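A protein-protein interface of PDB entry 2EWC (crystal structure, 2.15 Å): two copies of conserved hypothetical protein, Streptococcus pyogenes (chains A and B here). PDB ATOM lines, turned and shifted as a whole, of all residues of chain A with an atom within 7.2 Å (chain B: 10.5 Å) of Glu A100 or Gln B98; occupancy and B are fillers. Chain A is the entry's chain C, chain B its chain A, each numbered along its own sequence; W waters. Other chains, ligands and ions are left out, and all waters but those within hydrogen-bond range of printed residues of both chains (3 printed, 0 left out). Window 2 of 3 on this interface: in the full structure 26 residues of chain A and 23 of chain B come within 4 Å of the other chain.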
ATOM      1  N   LEU A  69     -20.413  10.423  32.425  1.00  0.00           N
ATOM      2  CA  LEU A  69     -20.855  10.640  31.060  1.00  0.00           C
ATOM      3  C   LEU A  69     -19.695  10.367  30.114  1.00  0.00           C
ATOM      4  O   LEU A  69     -18.624  10.959  30.272  1.00  0.00           O
ATOM      5  CB  LEU A  69     -21.335  12.085  30.863  1.00  0.00           C
ATOM      6  CG  LEU A  69     -22.350  12.693  31.871  1.00  0.00           C
ATOM      7  CD1 LEU A  69     -22.864  14.077  31.393  1.00  0.00           C
ATOM      8  CD2 LEU A  69     -23.543  11.768  32.099  1.00  0.00           C
ATOM      9  N   PHE A  70     -19.932   9.484  29.136  1.00  0.00           N
ATOM     10  CA  PHE A  70     -18.930   9.017  28.206  1.00  0.00           C
ATOM     11  C   PHE A  70     -19.377   9.323  26.823  1.00  0.00           C
ATOM     12  O   PHE A  70     -20.533   9.098  26.501  1.00  0.00           O
ATOM     13  CB  PHE A  70     -18.817   7.480  28.256  1.00  0.00           C
ATOM     14  CG  PHE A  70     -18.163   6.933  29.500  1.00  0.00           C
ATOM     15  CD1 PHE A  70     -16.802   6.583  29.493  1.00  0.00           C
ATOM     16  CD2 PHE A  70     -18.915   6.688  30.653  1.00  0.00           C
ATOM     17  CE1 PHE A  70     -16.203   6.047  30.622  1.00  0.00           C
ATOM     18  CE2 PHE A  70     -18.322   6.107  31.801  1.00  0.00           C
ATOM     19  CZ  PHE A  70     -16.970   5.808  31.788  1.00  0.00           C
ATOM     20  N   ARG A  71     -18.468   9.764  25.961  1.00  0.00           N
ATOM     21  CA  ARG A  71     -18.791   9.745  24.529  1.00  0.00           C
ATOM     22  C   ARG A  71     -18.946   8.277  24.008  1.00  0.00           C
ATOM     23  O   ARG A  71     -19.803   7.985  23.162  1.00  0.00           O
ATOM     24  CB  ARG A  71     -17.760  10.541  23.740  1.00  0.00           C
ATOM     25  CG  ARG A  71     -18.080  10.629  22.239  1.00  0.00           C
ATOM     26  CD  ARG A  71     -17.010  11.453  21.537  1.00  0.00           C
ATOM     27  NE  ARG A  71     -16.975  12.831  22.028  1.00  0.00           N
ATOM     28  CZ  ARG A  71     -17.754  13.821  21.594  1.00  0.00           C
ATOM     29  NH1 ARG A  71     -18.668  13.612  20.648  1.00  0.00           N
ATOM     30  NH2 ARG A  71     -17.611  15.035  22.115  1.00  0.00           N
ATOM     31  N   ILE A  97     -23.586   6.756  31.561  1.00  0.00           N
ATOM     32  CA  ILE A  97     -24.481   7.167  30.465  1.00  0.00           C
ATOM     33  C   ILE A  97     -23.585   7.498  29.272  1.00  0.00           C
ATOM     34  O   ILE A  97     -22.512   8.110  29.441  1.00  0.00           O
ATOM     35  CB  ILE A  97     -25.324   8.418  30.888  1.00  0.00           C
ATOM     36  CG1 ILE A  97     -26.350   8.019  31.952  1.00  0.00           C
ATOM     37  CG2 ILE A  97     -26.040   9.144  29.698  1.00  0.00           C
ATOM     38  CD1 ILE A  97     -26.679   9.214  32.878  1.00  0.00           C
ATOM     39  N   GLN A  98     -23.999   7.053  28.086  1.00  0.00           N
ATOM     40  CA  GLN A  98     -23.360   7.487  26.879  1.00  0.00           C
ATOM     41  C   GLN A  98     -24.133   8.680  26.370  1.00  0.00           C
ATOM     42  O   GLN A  98     -25.343   8.619  26.242  1.00  0.00           O
ATOM     43  CB  GLN A  98     -23.321   6.378  25.817  1.00  0.00           C
ATOM     44  CG  GLN A  98     -22.460   6.787  24.612  1.00  0.00           C
ATOM     45  CD  GLN A  98     -22.257   5.670  23.646  1.00  0.00           C
ATOM     46  OE1 GLN A  98     -21.531   4.730  23.932  1.00  0.00           O
ATOM     47  NE2 GLN A  98     -22.921   5.747  22.481  1.00  0.00           N
ATOM     48  N   THR A  99     -23.434   9.767  26.090  1.00  0.00           N
ATOM     49  CA  THR A  99     -24.077  10.960  25.586  1.00  0.00           C
ATOM     50  C   THR A  99     -23.178  11.718  24.609  1.00  0.00           C
ATOM     51  O   THR A  99     -21.937  11.649  24.692  1.00  0.00           O
ATOM     52  CB  THR A  99     -24.514  11.897  26.775  1.00  0.00           C
ATOM     53  OG1 THR A  99     -25.145  13.072  26.265  1.00  0.00           O
ATOM     54  CG2 THR A  99     -23.329  12.331  27.624  1.00  0.00           C
ATOM     55  N   GLU A 100     -23.798  12.475  23.713  1.00  0.00           N
ATOM     56  CA  GLU A 100     -23.068  13.502  22.993  1.00  0.00           C
ATOM     57  C   GLU A 100     -22.760  14.667  23.938  1.00  0.00           C
ATOM     58  O   GLU A 100     -23.439  14.849  24.954  1.00  0.00           O
ATOM     59  CB  GLU A 100     -23.843  13.980  21.756  1.00  0.00           C
ATOM     60  CG  GLU A 100     -23.995  12.889  20.671  1.00  0.00           C
ATOM     61  CD  GLU A 100     -22.680  12.578  19.938  1.00  0.00           C
ATOM     62  OE1 GLU A 100     -22.061  13.502  19.349  1.00  0.00           O
ATOM     63  OE2 GLU A 100     -22.265  11.400  19.941  1.00  0.00           O
ATOM     64  N   PHE A 101     -21.702  15.407  23.633  1.00  0.00           N
ATOM     65  CA  PHE A 101     -21.386  16.650  24.338  1.00  0.00           C
ATOM     66  C   PHE A 101     -21.522  17.863  23.393  1.00  0.00           C
ATOM     67  O   PHE A 101     -21.384  17.731  22.157  1.00  0.00           O
ATOM     68  CB  PHE A 101     -19.963  16.587  24.896  1.00  0.00           C
ATOM     69  CG  PHE A 101     -19.751  15.481  25.909  1.00  0.00           C
ATOM     70  CD1 PHE A 101     -20.352  15.540  27.170  1.00  0.00           C
ATOM     71  CD2 PHE A 101     -18.947  14.387  25.599  1.00  0.00           C
ATOM     72  CE1 PHE A 101     -20.175  14.522  28.104  1.00  0.00           C
ATOM     73  CE2 PHE A 101     -18.721  13.379  26.537  1.00  0.00           C
ATOM     74  CZ  PHE A 101     -19.341  13.441  27.795  1.00  0.00           C
ATOM     75  N   ALA A 102     -21.774  19.035  23.963  1.00  0.00           N
ATOM     76  CA  ALA A 102     -21.672  20.286  23.190  1.00  0.00           C
ATOM     77  C   ALA A 102     -20.188  20.701  22.970  1.00  0.00           C
ATOM     78  O   ALA A 102     -19.818  21.841  23.165  1.00  0.00           O
ATOM     79  CB  ALA A 102     -22.480  21.426  23.879  1.00  0.00           C
ATOM     80  N   HIS A 103     -19.358  19.737  22.573  1.00  0.00           N
ATOM     81  CA  HIS A 103     -17.949  19.967  22.225  1.00  0.00           C
ATOM     82  C   HIS A 103     -17.568  18.840  21.276  1.00  0.00           C
ATOM     83  O   HIS A 103     -18.106  17.726  21.373  1.00  0.00           O
ATOM     84  CB  HIS A 103     -17.033  19.963  23.466  1.00  0.00           C
ATOM     85  CG  HIS A 103     -15.570  20.043  23.143  1.00  0.00           C
ATOM     86  ND1 HIS A 103     -14.837  21.204  23.262  1.00  0.00           N
ATOM     87  CD2 HIS A 103     -14.706  19.099  22.694  1.00  0.00           C
ATOM     88  CE1 HIS A 103     -13.588  20.971  22.899  1.00  0.00           C
ATOM     89  NE2 HIS A 103     -13.488  19.702  22.539  1.00  0.00           N
ATOM     90  N   GLY A 105     -15.824  15.788  19.195  1.00  0.00           N
ATOM     91  CA  GLY A 105     -15.112  14.549  19.523  1.00  0.00           C
ATOM     92  C   GLY A 105     -13.868  14.475  18.653  1.00  0.00           C
ATOM     93  O   GLY A 105     -13.297  15.498  18.316  1.00  0.00           O
ATOM     94  N   GLN A 113     -17.051  13.284  31.214  1.00  0.00           N
ATOM     95  CA  GLN A 113     -17.359  14.168  32.345  1.00  0.00           C
ATOM     96  C   GLN A 113     -17.909  13.318  33.467  1.00  0.00           C
ATOM     97  O   GLN A 113     -18.393  12.212  33.245  1.00  0.00           O
ATOM     98  CB  GLN A 113     -18.448  15.171  31.985  1.00  0.00           C
ATOM     99  CG  GLN A 113     -18.177  15.983  30.768  1.00  0.00           C
ATOM    100  CD  GLN A 113     -19.292  16.987  30.514  1.00  0.00           C
ATOM    101  OE1 GLN A 113     -20.436  16.781  30.919  1.00  0.00           O
ATOM    102  NE2 GLN A 113     -18.954  18.082  29.880  1.00  0.00           N
ATOM    103  N   ASP B  67     -30.582  18.278  36.389  1.00  0.00           N
ATOM    104  CA  ASP B  67     -30.165  17.503  35.194  1.00  0.00           C
ATOM    105  C   ASP B  67     -30.963  17.991  33.992  1.00  0.00           C
ATOM    106  O   ASP B  67     -32.191  17.994  34.036  1.00  0.00           O
ATOM    107  CB  ASP B  67     -30.424  16.019  35.385  1.00  0.00           C
ATOM    108  CG  ASP B  67     -29.481  15.382  36.404  1.00  0.00           C
ATOM    109  OD1 ASP B  67     -28.314  15.831  36.506  1.00  0.00           O
ATOM    110  OD2 ASP B  67     -29.898  14.424  37.107  1.00  0.00           O
ATOM    111  N   CYS B  68     -30.269  18.402  32.934  1.00  0.00           N
ATOM    112  CA  CYS B  68     -30.904  18.951  31.731  1.00  0.00           C
ATOM    113  C   CYS B  68     -30.819  17.965  30.543  1.00  0.00           C
ATOM    114  O   CYS B  68     -29.729  17.498  30.161  1.00  0.00           O
ATOM    115  CB  CYS B  68     -30.234  20.269  31.366  1.00  0.00           C
ATOM    116  SG  CYS B  68     -29.915  21.346  32.792  1.00  0.00           S
ATOM    117  N   LEU B  69     -31.977  17.649  29.984  1.00  0.00           N
ATOM    118  CA  LEU B  69     -32.126  16.656  28.933  1.00  0.00           C
ATOM    119  C   LEU B  69     -32.466  17.355  27.616  1.00  0.00           C
ATOM    120  O   LEU B  69     -33.501  18.060  27.490  1.00  0.00           O
ATOM    121  CB  LEU B  69     -33.256  15.703  29.316  1.00  0.00           C
ATOM    122  CG  LEU B  69     -32.891  14.456  30.152  1.00  0.00           C
ATOM    123  CD1 LEU B  69     -31.762  14.581  31.169  1.00  0.00           C
ATOM    124  CD2 LEU B  69     -34.156  13.880  30.785  1.00  0.00           C
ATOM    125  N   PHE B  70     -31.586  17.191  26.648  1.00  0.00           N
ATOM    126  CA  PHE B  70     -31.776  17.820  25.334  1.00  0.00           C
ATOM    127  C   PHE B  70     -31.958  16.772  24.265  1.00  0.00           C
ATOM    128  O   PHE B  70     -31.345  15.713  24.312  1.00  0.00           O
ATOM    129  CB  PHE B  70     -30.546  18.634  24.946  1.00  0.00           C
ATOM    130  CG  PHE B  70     -30.294  19.829  25.825  1.00  0.00           C
ATOM    131  CD1 PHE B  70     -30.779  21.072  25.471  1.00  0.00           C
ATOM    132  CD2 PHE B  70     -29.522  19.709  26.981  1.00  0.00           C
ATOM    133  CE1 PHE B  70     -30.512  22.208  26.275  1.00  0.00           C
ATOM    134  CE2 PHE B  70     -29.244  20.828  27.806  1.00  0.00           C
ATOM    135  CZ  PHE B  70     -29.748  22.075  27.449  1.00  0.00           C
ATOM    136  N   ARG B  71     -32.775  17.086  23.277  1.00  0.00           N
ATOM    137  CA  ARG B  71     -32.769  16.313  22.046  1.00  0.00           C
ATOM    138  C   ARG B  71     -31.478  16.640  21.299  1.00  0.00           C
ATOM    139  O   ARG B  71     -30.905  15.785  20.601  1.00  0.00           O
ATOM    140  CB  ARG B  71     -33.999  16.681  21.183  1.00  0.00           C
ATOM    141  CG  ARG B  71     -34.165  15.752  19.997  1.00  0.00           C
ATOM    142  CD  ARG B  71     -35.500  15.980  19.236  1.00  0.00           C
ATOM    143  NE  ARG B  71     -36.648  15.590  20.042  1.00  0.00           N
ATOM    144  CZ  ARG B  71     -37.163  14.358  20.103  1.00  0.00           C
ATOM    145  NH1 ARG B  71     -36.641  13.368  19.399  1.00  0.00           N
ATOM    146  NH2 ARG B  71     -38.211  14.117  20.873  1.00  0.00           N
ATOM    147  N   ASP B  72     -31.027  17.896  21.446  1.00  0.00           N
ATOM    148  CA  ASP B  72     -29.806  18.375  20.806  1.00  0.00           C
ATOM    149  C   ASP B  72     -29.006  19.169  21.837  1.00  0.00           C
ATOM    150  O   ASP B  72     -29.333  20.306  22.144  1.00  0.00           O
ATOM    151  CB  ASP B  72     -30.147  19.249  19.573  1.00  0.00           C
ATOM    152  CG  ASP B  72     -28.885  19.819  18.864  1.00  0.00           C
ATOM    153  OD1 ASP B  72     -27.739  19.586  19.333  1.00  0.00           O
ATOM    154  OD2 ASP B  72     -29.036  20.503  17.817  1.00  0.00           O
ATOM    155  N   VAL B  73     -27.953  18.557  22.353  1.00  0.00           N
ATOM    156  CA  VAL B  73     -27.207  19.113  23.459  1.00  0.00           C
ATOM    157  C   VAL B  73     -26.443  20.385  23.090  1.00  0.00           C
ATOM    158  O   VAL B  73     -26.087  21.182  23.986  1.00  0.00           O
ATOM    159  CB  VAL B  73     -26.292  18.041  24.130  1.00  0.00           C
ATOM    160  CG1 VAL B  73     -25.041  17.776  23.305  1.00  0.00           C
ATOM    161  CG2 VAL B  73     -25.975  18.447  25.549  1.00  0.00           C
ATOM    162  N   TRP B  74     -26.230  20.597  21.784  1.00  0.00           N
ATOM    163  CA  TRP B  74     -25.630  21.838  21.293  1.00  0.00           C
ATOM    164  C   TRP B  74     -26.527  23.059  21.556  1.00  0.00           C
ATOM    165  O   TRP B  74     -26.152  24.193  21.281  1.00  0.00           O
ATOM    166  CB  TRP B  74     -25.272  21.734  19.815  1.00  0.00           C
ATOM    167  CG  TRP B  74     -24.121  20.766  19.534  1.00  0.00           C
ATOM    168  CD1 TRP B  74     -24.220  19.432  19.176  1.00  0.00           C
ATOM    169  CD2 TRP B  74     -22.717  21.058  19.596  1.00  0.00           C
ATOM    170  NE1 TRP B  74     -22.958  18.900  19.007  1.00  0.00           N
ATOM    171  CE2 TRP B  74     -22.024  19.875  19.253  1.00  0.00           C
ATOM    172  CE3 TRP B  74     -21.978  22.215  19.885  1.00  0.00           C
ATOM    173  CZ2 TRP B  74     -20.618  19.815  19.195  1.00  0.00           C
ATOM    174  CZ3 TRP B  74     -20.595  22.160  19.821  1.00  0.00           C
ATOM    175  CH2 TRP B  74     -19.928  20.968  19.475  1.00  0.00           C
ATOM    176  N   ASN B  75     -27.711  22.820  22.090  1.00  0.00           N
ATOM    177  CA  ASN B  75     -28.542  23.908  22.580  1.00  0.00           C
ATOM    178  C   ASN B  75     -28.189  24.386  23.978  1.00  0.00           C
ATOM    179  O   ASN B  75     -28.896  25.229  24.523  1.00  0.00           O
ATOM    180  CB  ASN B  75     -30.015  23.512  22.545  1.00  0.00           C
ATOM    181  CG  ASN B  75     -30.574  23.540  21.135  1.00  0.00           C
ATOM    182  OD1 ASN B  75     -30.271  24.442  20.356  1.00  0.00           O
ATOM    183  ND2 ASN B  75     -31.371  22.549  20.799  1.00  0.00           N
ATOM    184  N   ILE B  76     -27.130  23.857  24.586  1.00  0.00           N
ATOM    185  CA  ILE B  76     -26.753  24.369  25.917  1.00  0.00           C
ATOM    186  C   ILE B  76     -26.666  25.920  25.969  1.00  0.00           C
ATOM    187  O   ILE B  76     -27.186  26.504  26.911  1.00  0.00           O
ATOM    188  CB  ILE B  76     -25.480  23.735  26.482  1.00  0.00           C
ATOM    189  CG1 ILE B  76     -25.781  22.348  27.061  1.00  0.00           C
ATOM    190  CG2 ILE B  76     -24.892  24.619  27.613  1.00  0.00           C
ATOM    191  CD1 ILE B  76     -24.499  21.458  27.217  1.00  0.00           C
ATOM    192  N   LYS B  95     -25.682  18.947  35.155  1.00  0.00           N
ATOM    193  CA  LYS B  95     -25.115  18.318  34.005  1.00  0.00           C
ATOM    194  C   LYS B  95     -26.154  18.310  32.894  1.00  0.00           C
ATOM    195  O   LYS B  95     -27.356  18.341  33.160  1.00  0.00           O
ATOM    196  CB  LYS B  95     -24.605  16.917  34.349  1.00  0.00           C
ATOM    197  CG  LYS B  95     -25.704  15.934  34.645  1.00  0.00           C
ATOM    198  CD  LYS B  95     -25.124  14.524  34.795  1.00  0.00           C
ATOM    199  CE  LYS B  95     -26.174  13.591  35.374  1.00  0.00           C
ATOM    200  NZ  LYS B  95     -26.301  13.968  36.776  1.00  0.00           N
ATOM    201  N   SER B  96     -25.672  18.287  31.659  1.00  0.00           N
ATOM    202  CA  SER B  96     -26.513  18.137  30.484  1.00  0.00           C
ATOM    203  C   SER B  96     -26.263  16.802  29.733  1.00  0.00           C
ATOM    204  O   SER B  96     -25.124  16.332  29.613  1.00  0.00           O
ATOM    205  CB  SER B  96     -26.278  19.318  29.552  1.00  0.00           C
ATOM    206  OG  SER B  96     -26.537  20.527  30.244  1.00  0.00           O
ATOM    207  N   ILE B  97     -27.349  16.218  29.236  1.00  0.00           N
ATOM    208  CA  ILE B  97     -27.338  14.924  28.544  1.00  0.00           C
ATOM    209  C   ILE B  97     -28.165  15.085  27.281  1.00  0.00           C
ATOM    210  O   ILE B  97     -29.214  15.761  27.272  1.00  0.00           O
ATOM    211  CB  ILE B  97     -27.969  13.841  29.478  1.00  0.00           C
ATOM    212  CG1 ILE B  97     -26.977  13.423  30.568  1.00  0.00           C
ATOM    213  CG2 ILE B  97     -28.435  12.608  28.755  1.00  0.00           C
ATOM    214  CD1 ILE B  97     -27.748  12.853  31.761  1.00  0.00           C
ATOM    215  N   GLN B  98     -27.683  14.497  26.201  1.00  0.00           N
ATOM    216  CA  GLN B  98     -28.462  14.417  25.003  1.00  0.00           C
ATOM    217  C   GLN B  98     -29.142  13.058  25.029  1.00  0.00           C
ATOM    218  O   GLN B  98     -28.505  12.050  25.330  1.00  0.00           O
ATOM    219  CB  GLN B  98     -27.580  14.562  23.762  1.00  0.00           C
ATOM    220  CG  GLN B  98     -28.375  14.412  22.484  1.00  0.00           C
ATOM    221  CD  GLN B  98     -27.626  14.870  21.242  1.00  0.00           C
ATOM    222  OE1 GLN B  98     -27.244  16.030  21.123  1.00  0.00           O
ATOM    223  NE2 GLN B  98     -27.415  13.953  20.315  1.00  0.00           N
ATOM    224  N   THR B  99     -30.438  13.027  24.766  1.00  0.00           N
ATOM    225  CA  THR B  99     -31.201  11.771  24.829  1.00  0.00           C
ATOM    226  C   THR B  99     -32.413  11.842  23.902  1.00  0.00           C
ATOM    227  O   THR B  99     -32.925  12.925  23.609  1.00  0.00           O
ATOM    228  CB  THR B  99     -31.697  11.425  26.292  1.00  0.00           C
ATOM    229  OG1 THR B  99     -32.432  10.192  26.278  1.00  0.00           O
ATOM    230  CG2 THR B  99     -32.621  12.512  26.830  1.00  0.00           C
ATOM    231  N   GLU B 100     -32.865  10.686  23.442  1.00  0.00           N
ATOM    232  CA  GLU B 100     -34.175  10.595  22.815  1.00  0.00           C
ATOM    233  C   GLU B 100     -35.232  10.661  23.904  1.00  0.00           C
ATOM    234  O   GLU B 100     -34.942  10.343  25.073  1.00  0.00           O
ATOM    235  CB  GLU B 100     -34.310   9.269  22.069  1.00  0.00           C
ATOM    236  CG  GLU B 100     -33.263   9.092  21.012  1.00  0.00           C
ATOM    237  CD  GLU B 100     -33.423  10.087  19.860  1.00  0.00           C
ATOM    238  OE1 GLU B 100     -34.582  10.491  19.541  1.00  0.00           O
ATOM    239  OE2 GLU B 100     -32.380  10.462  19.276  1.00  0.00           O
ATOM    240  N   PHE B 101     -36.442  11.044  23.508  1.00  0.00           N
ATOM    241  CA  PHE B 101     -37.611  11.040  24.379  1.00  0.00           C
ATOM    242  C   PHE B 101     -38.670  10.102  23.815  1.00  0.00           C
ATOM    243  O   PHE B 101     -38.673   9.830  22.622  1.00  0.00           O
ATOM    244  CB  PHE B 101     -38.190  12.435  24.425  1.00  0.00           C
ATOM    245  CG  PHE B 101     -37.243  13.476  24.999  1.00  0.00           C
ATOM    246  CD1 PHE B 101     -36.827  13.409  26.328  1.00  0.00           C
ATOM    247  CD2 PHE B 101     -36.791  14.516  24.209  1.00  0.00           C
ATOM    248  CE1 PHE B 101     -35.956  14.388  26.862  1.00  0.00           C
ATOM    249  CE2 PHE B 101     -35.950  15.507  24.726  1.00  0.00           C
ATOM    250  CZ  PHE B 101     -35.535  15.438  26.056  1.00  0.00           C
ATOM    251  N   LEU B 110     -41.018  17.522  21.197  1.00  0.00           N
ATOM    252  CA  LEU B 110     -40.381  17.771  22.486  1.00  0.00           C
ATOM    253  C   LEU B 110     -38.866  17.893  22.300  1.00  0.00           C
ATOM    254  O   LEU B 110     -38.256  17.082  21.608  1.00  0.00           O
ATOM    255  CB  LEU B 110     -40.722  16.643  23.461  1.00  0.00           C
ATOM    256  CG  LEU B 110     -40.048  16.735  24.849  1.00  0.00           C
ATOM    257  CD1 LEU B 110     -40.433  18.056  25.505  1.00  0.00           C
ATOM    258  CD2 LEU B 110     -40.473  15.553  25.757  1.00  0.00           C
ATOM    259  N   LEU B 111     -38.255  18.902  22.915  1.00  0.00           N
ATOM    260  CA  LEU B 111     -36.844  19.193  22.689  1.00  0.00           C
ATOM    261  C   LEU B 111     -36.009  19.251  23.948  1.00  0.00           C
ATOM    262  O   LEU B 111     -34.762  19.284  23.876  1.00  0.00           O
ATOM    263  CB  LEU B 111     -36.696  20.535  21.931  1.00  0.00           C
ATOM    264  CG  LEU B 111     -37.485  20.724  20.646  1.00  0.00           C
ATOM    265  CD1 LEU B 111     -37.244  22.107  20.085  1.00  0.00           C
ATOM    266  CD2 LEU B 111     -37.035  19.663  19.622  1.00  0.00           C
ATOM    267  N   PHE B 112     -36.687  19.293  25.092  1.00  0.00           N
ATOM    268  CA  PHE B 112     -36.045  19.629  26.363  1.00  0.00           C
ATOM    269  C   PHE B 112     -36.848  19.204  27.574  1.00  0.00           C
ATOM    270  O   PHE B 112     -38.053  19.442  27.628  1.00  0.00           O
ATOM    271  CB  PHE B 112     -35.780  21.138  26.436  1.00  0.00           C
ATOM    272  CG  PHE B 112     -35.030  21.573  27.682  1.00  0.00           C
ATOM    273  CD1 PHE B 112     -33.647  21.478  27.742  1.00  0.00           C
ATOM    274  CD2 PHE B 112     -35.713  22.114  28.775  1.00  0.00           C
ATOM    275  CE1 PHE B 112     -32.945  21.878  28.881  1.00  0.00           C
ATOM    276  CE2 PHE B 112     -35.018  22.541  29.916  1.00  0.00           C
ATOM    277  CZ  PHE B 112     -33.627  22.414  29.971  1.00  0.00           C
ATOM    278  N   GLN B 113     -36.183  18.570  28.540  1.00  0.00           N
ATOM    279  CA  GLN B 113     -36.735  18.374  29.884  1.00  0.00           C
ATOM    280  C   GLN B 113     -35.674  18.730  30.923  1.00  0.00           C
ATOM    281  O   GLN B 113     -34.482  18.677  30.646  1.00  0.00           O
ATOM    282  CB  GLN B 113     -37.159  16.929  30.129  1.00  0.00           C
ATOM    283  CG  GLN B 113     -38.089  16.335  29.105  1.00  0.00           C
ATOM    284  CD  GLN B 113     -38.435  14.888  29.441  1.00  0.00           C
ATOM    285  OE1 GLN B 113     -37.678  14.209  30.137  1.00  0.00           O
ATOM    286  NE2 GLN B 113     -39.579  14.413  28.950  1.00  0.00           N
HETATM  287  O   HOH W   1     -22.888  18.073  31.168  1.00  0.00           O
HETATM  288  O   HOH W   2     -23.622  16.525  27.214  1.00  0.00           O
HETATM  289  O   HOH W   3     -26.449  11.024  23.106  1.00  0.00           O
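The backbone NH of Gln B98 sits at hydrogen-bond distance from the side-chain hydroxyl of Thr A99, at 2.9 Å.
O of Cys B68 sits at hydrogen-bond distance from N of Ile B97, 2.9 Å away. N of Phe B70 lies within hydrogen-bond range of O of Ile B97, 2.8 Å away. The side-chain carboxylate of Asp B72 sits at hydrogen-bond distance from the backbone NH of Trp B74 (3.1 Å). N of Val B73 is in hydrogen-bond range of OE1 of Gln B98 (2.9 Å). N of Leu A69 is in hydrogen-bond range of O of Gln A113 (2.8 Å). N of Phe A70 is in hydrogen-bond range of O of Ile A97, at 2.9 Å.
CD1 of Leu A69 touches O of Ser B96 (3.7 Å). Ile B97 touches Ile A97 (CD1 to CD1, 3.95 Å). Glu A100 touches Val B73. NE2 of Gln B98 touches CG of Glu A100, 3.6 Å away. Val B73 touches Phe A101. Phe A101 touches Trp B74. CG1 of Val B73 touches N of Ala A102, at 3.6 Å. Ala A102 touches Trp B74 (O to CZ3, 3.4 Å). Ala A102 touches Ile B76. CH2 of Trp B74 touches N of His A103 (3.4 Å).
Of chain B, only Val B73 and Gln B98 come within 4 Å of Glu A100. Gln B98 touches just these residues of chain A: Thr A99 and Glu A100. No residue of chain B comes within 4 Å of Arg A71. Printed residues of chain B within 4 Å of Thr A99: Ile B97 and Gln B98. Phe A101 touches just these residues of chain B: Val B73 and Trp B74. Printed residues of chain B within 4 Å of His A103: Trp B74. Printed residues of chain A within 4 Å of Val B73: Glu A100 (3.7 Å), Phe A101 (3.5 Å) and Ala A102 (3.6 Å). Thr B99 touches none of the printed residues of chain A. Gln B113 touches none of the printed residues of chain A. The nearest residue of chain B that does not touch Glu A100 is Ser B96 (5.2 Å).
Of the 21 printed residues of chain B, 6 touch a printed residue of chain A. Hydrophobic or aromatic side chains of chain B that line the printed part of chain A: Val B73, Trp B74, Ile B76 and Ile B97. Printed residues of chain A that touch a printed residue of chain B: Leu A69, Ile A97, Thr A99, Glu A100, Phe A101, Ala A102 and His A103. Hydrophobic or aromatic side chains of chain A within 4 Å of the printed part of chain B: Leu A69, Ile A97 and Ala A102. Along chain A the printed residues that touch a printed residue of chain B span positions 69 to 103. Among the printed residues, no Asp or Glu carboxylate lies within 4 Å of a Lys or Arg side-chain nitrogen of the other chain.
Ile B97 touches its own counterpart, Ile A97. Thr A99 touches Ile B97, but with the chains exchanged Ile A97 does not touch Thr B99 (7.0 Å). Thr A99 touches Gln B98, but with the chains exchanged Gln A98 does not touch Thr B99 (6.8 Å). Glu A100 touches Gln B98, but with the chains exchanged Gln A98 does not touch Glu B100 (8.3 Å). Of the 12 pairs that touch across the chains among the printed residues, 1 has its exchanged pair printed and touching as well.
Water W1 bridges OE1 of Gln A113 (2.8 Å) and N of Ser B96 (2.8 Å). Water W2 bridges O of Glu A100 and O of Ser B96. Water W3 bridges the backbone NH of Glu A100 (3.1 Å) and the backbone carbonyl oxygen of Gln B98 (3.2 Å).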
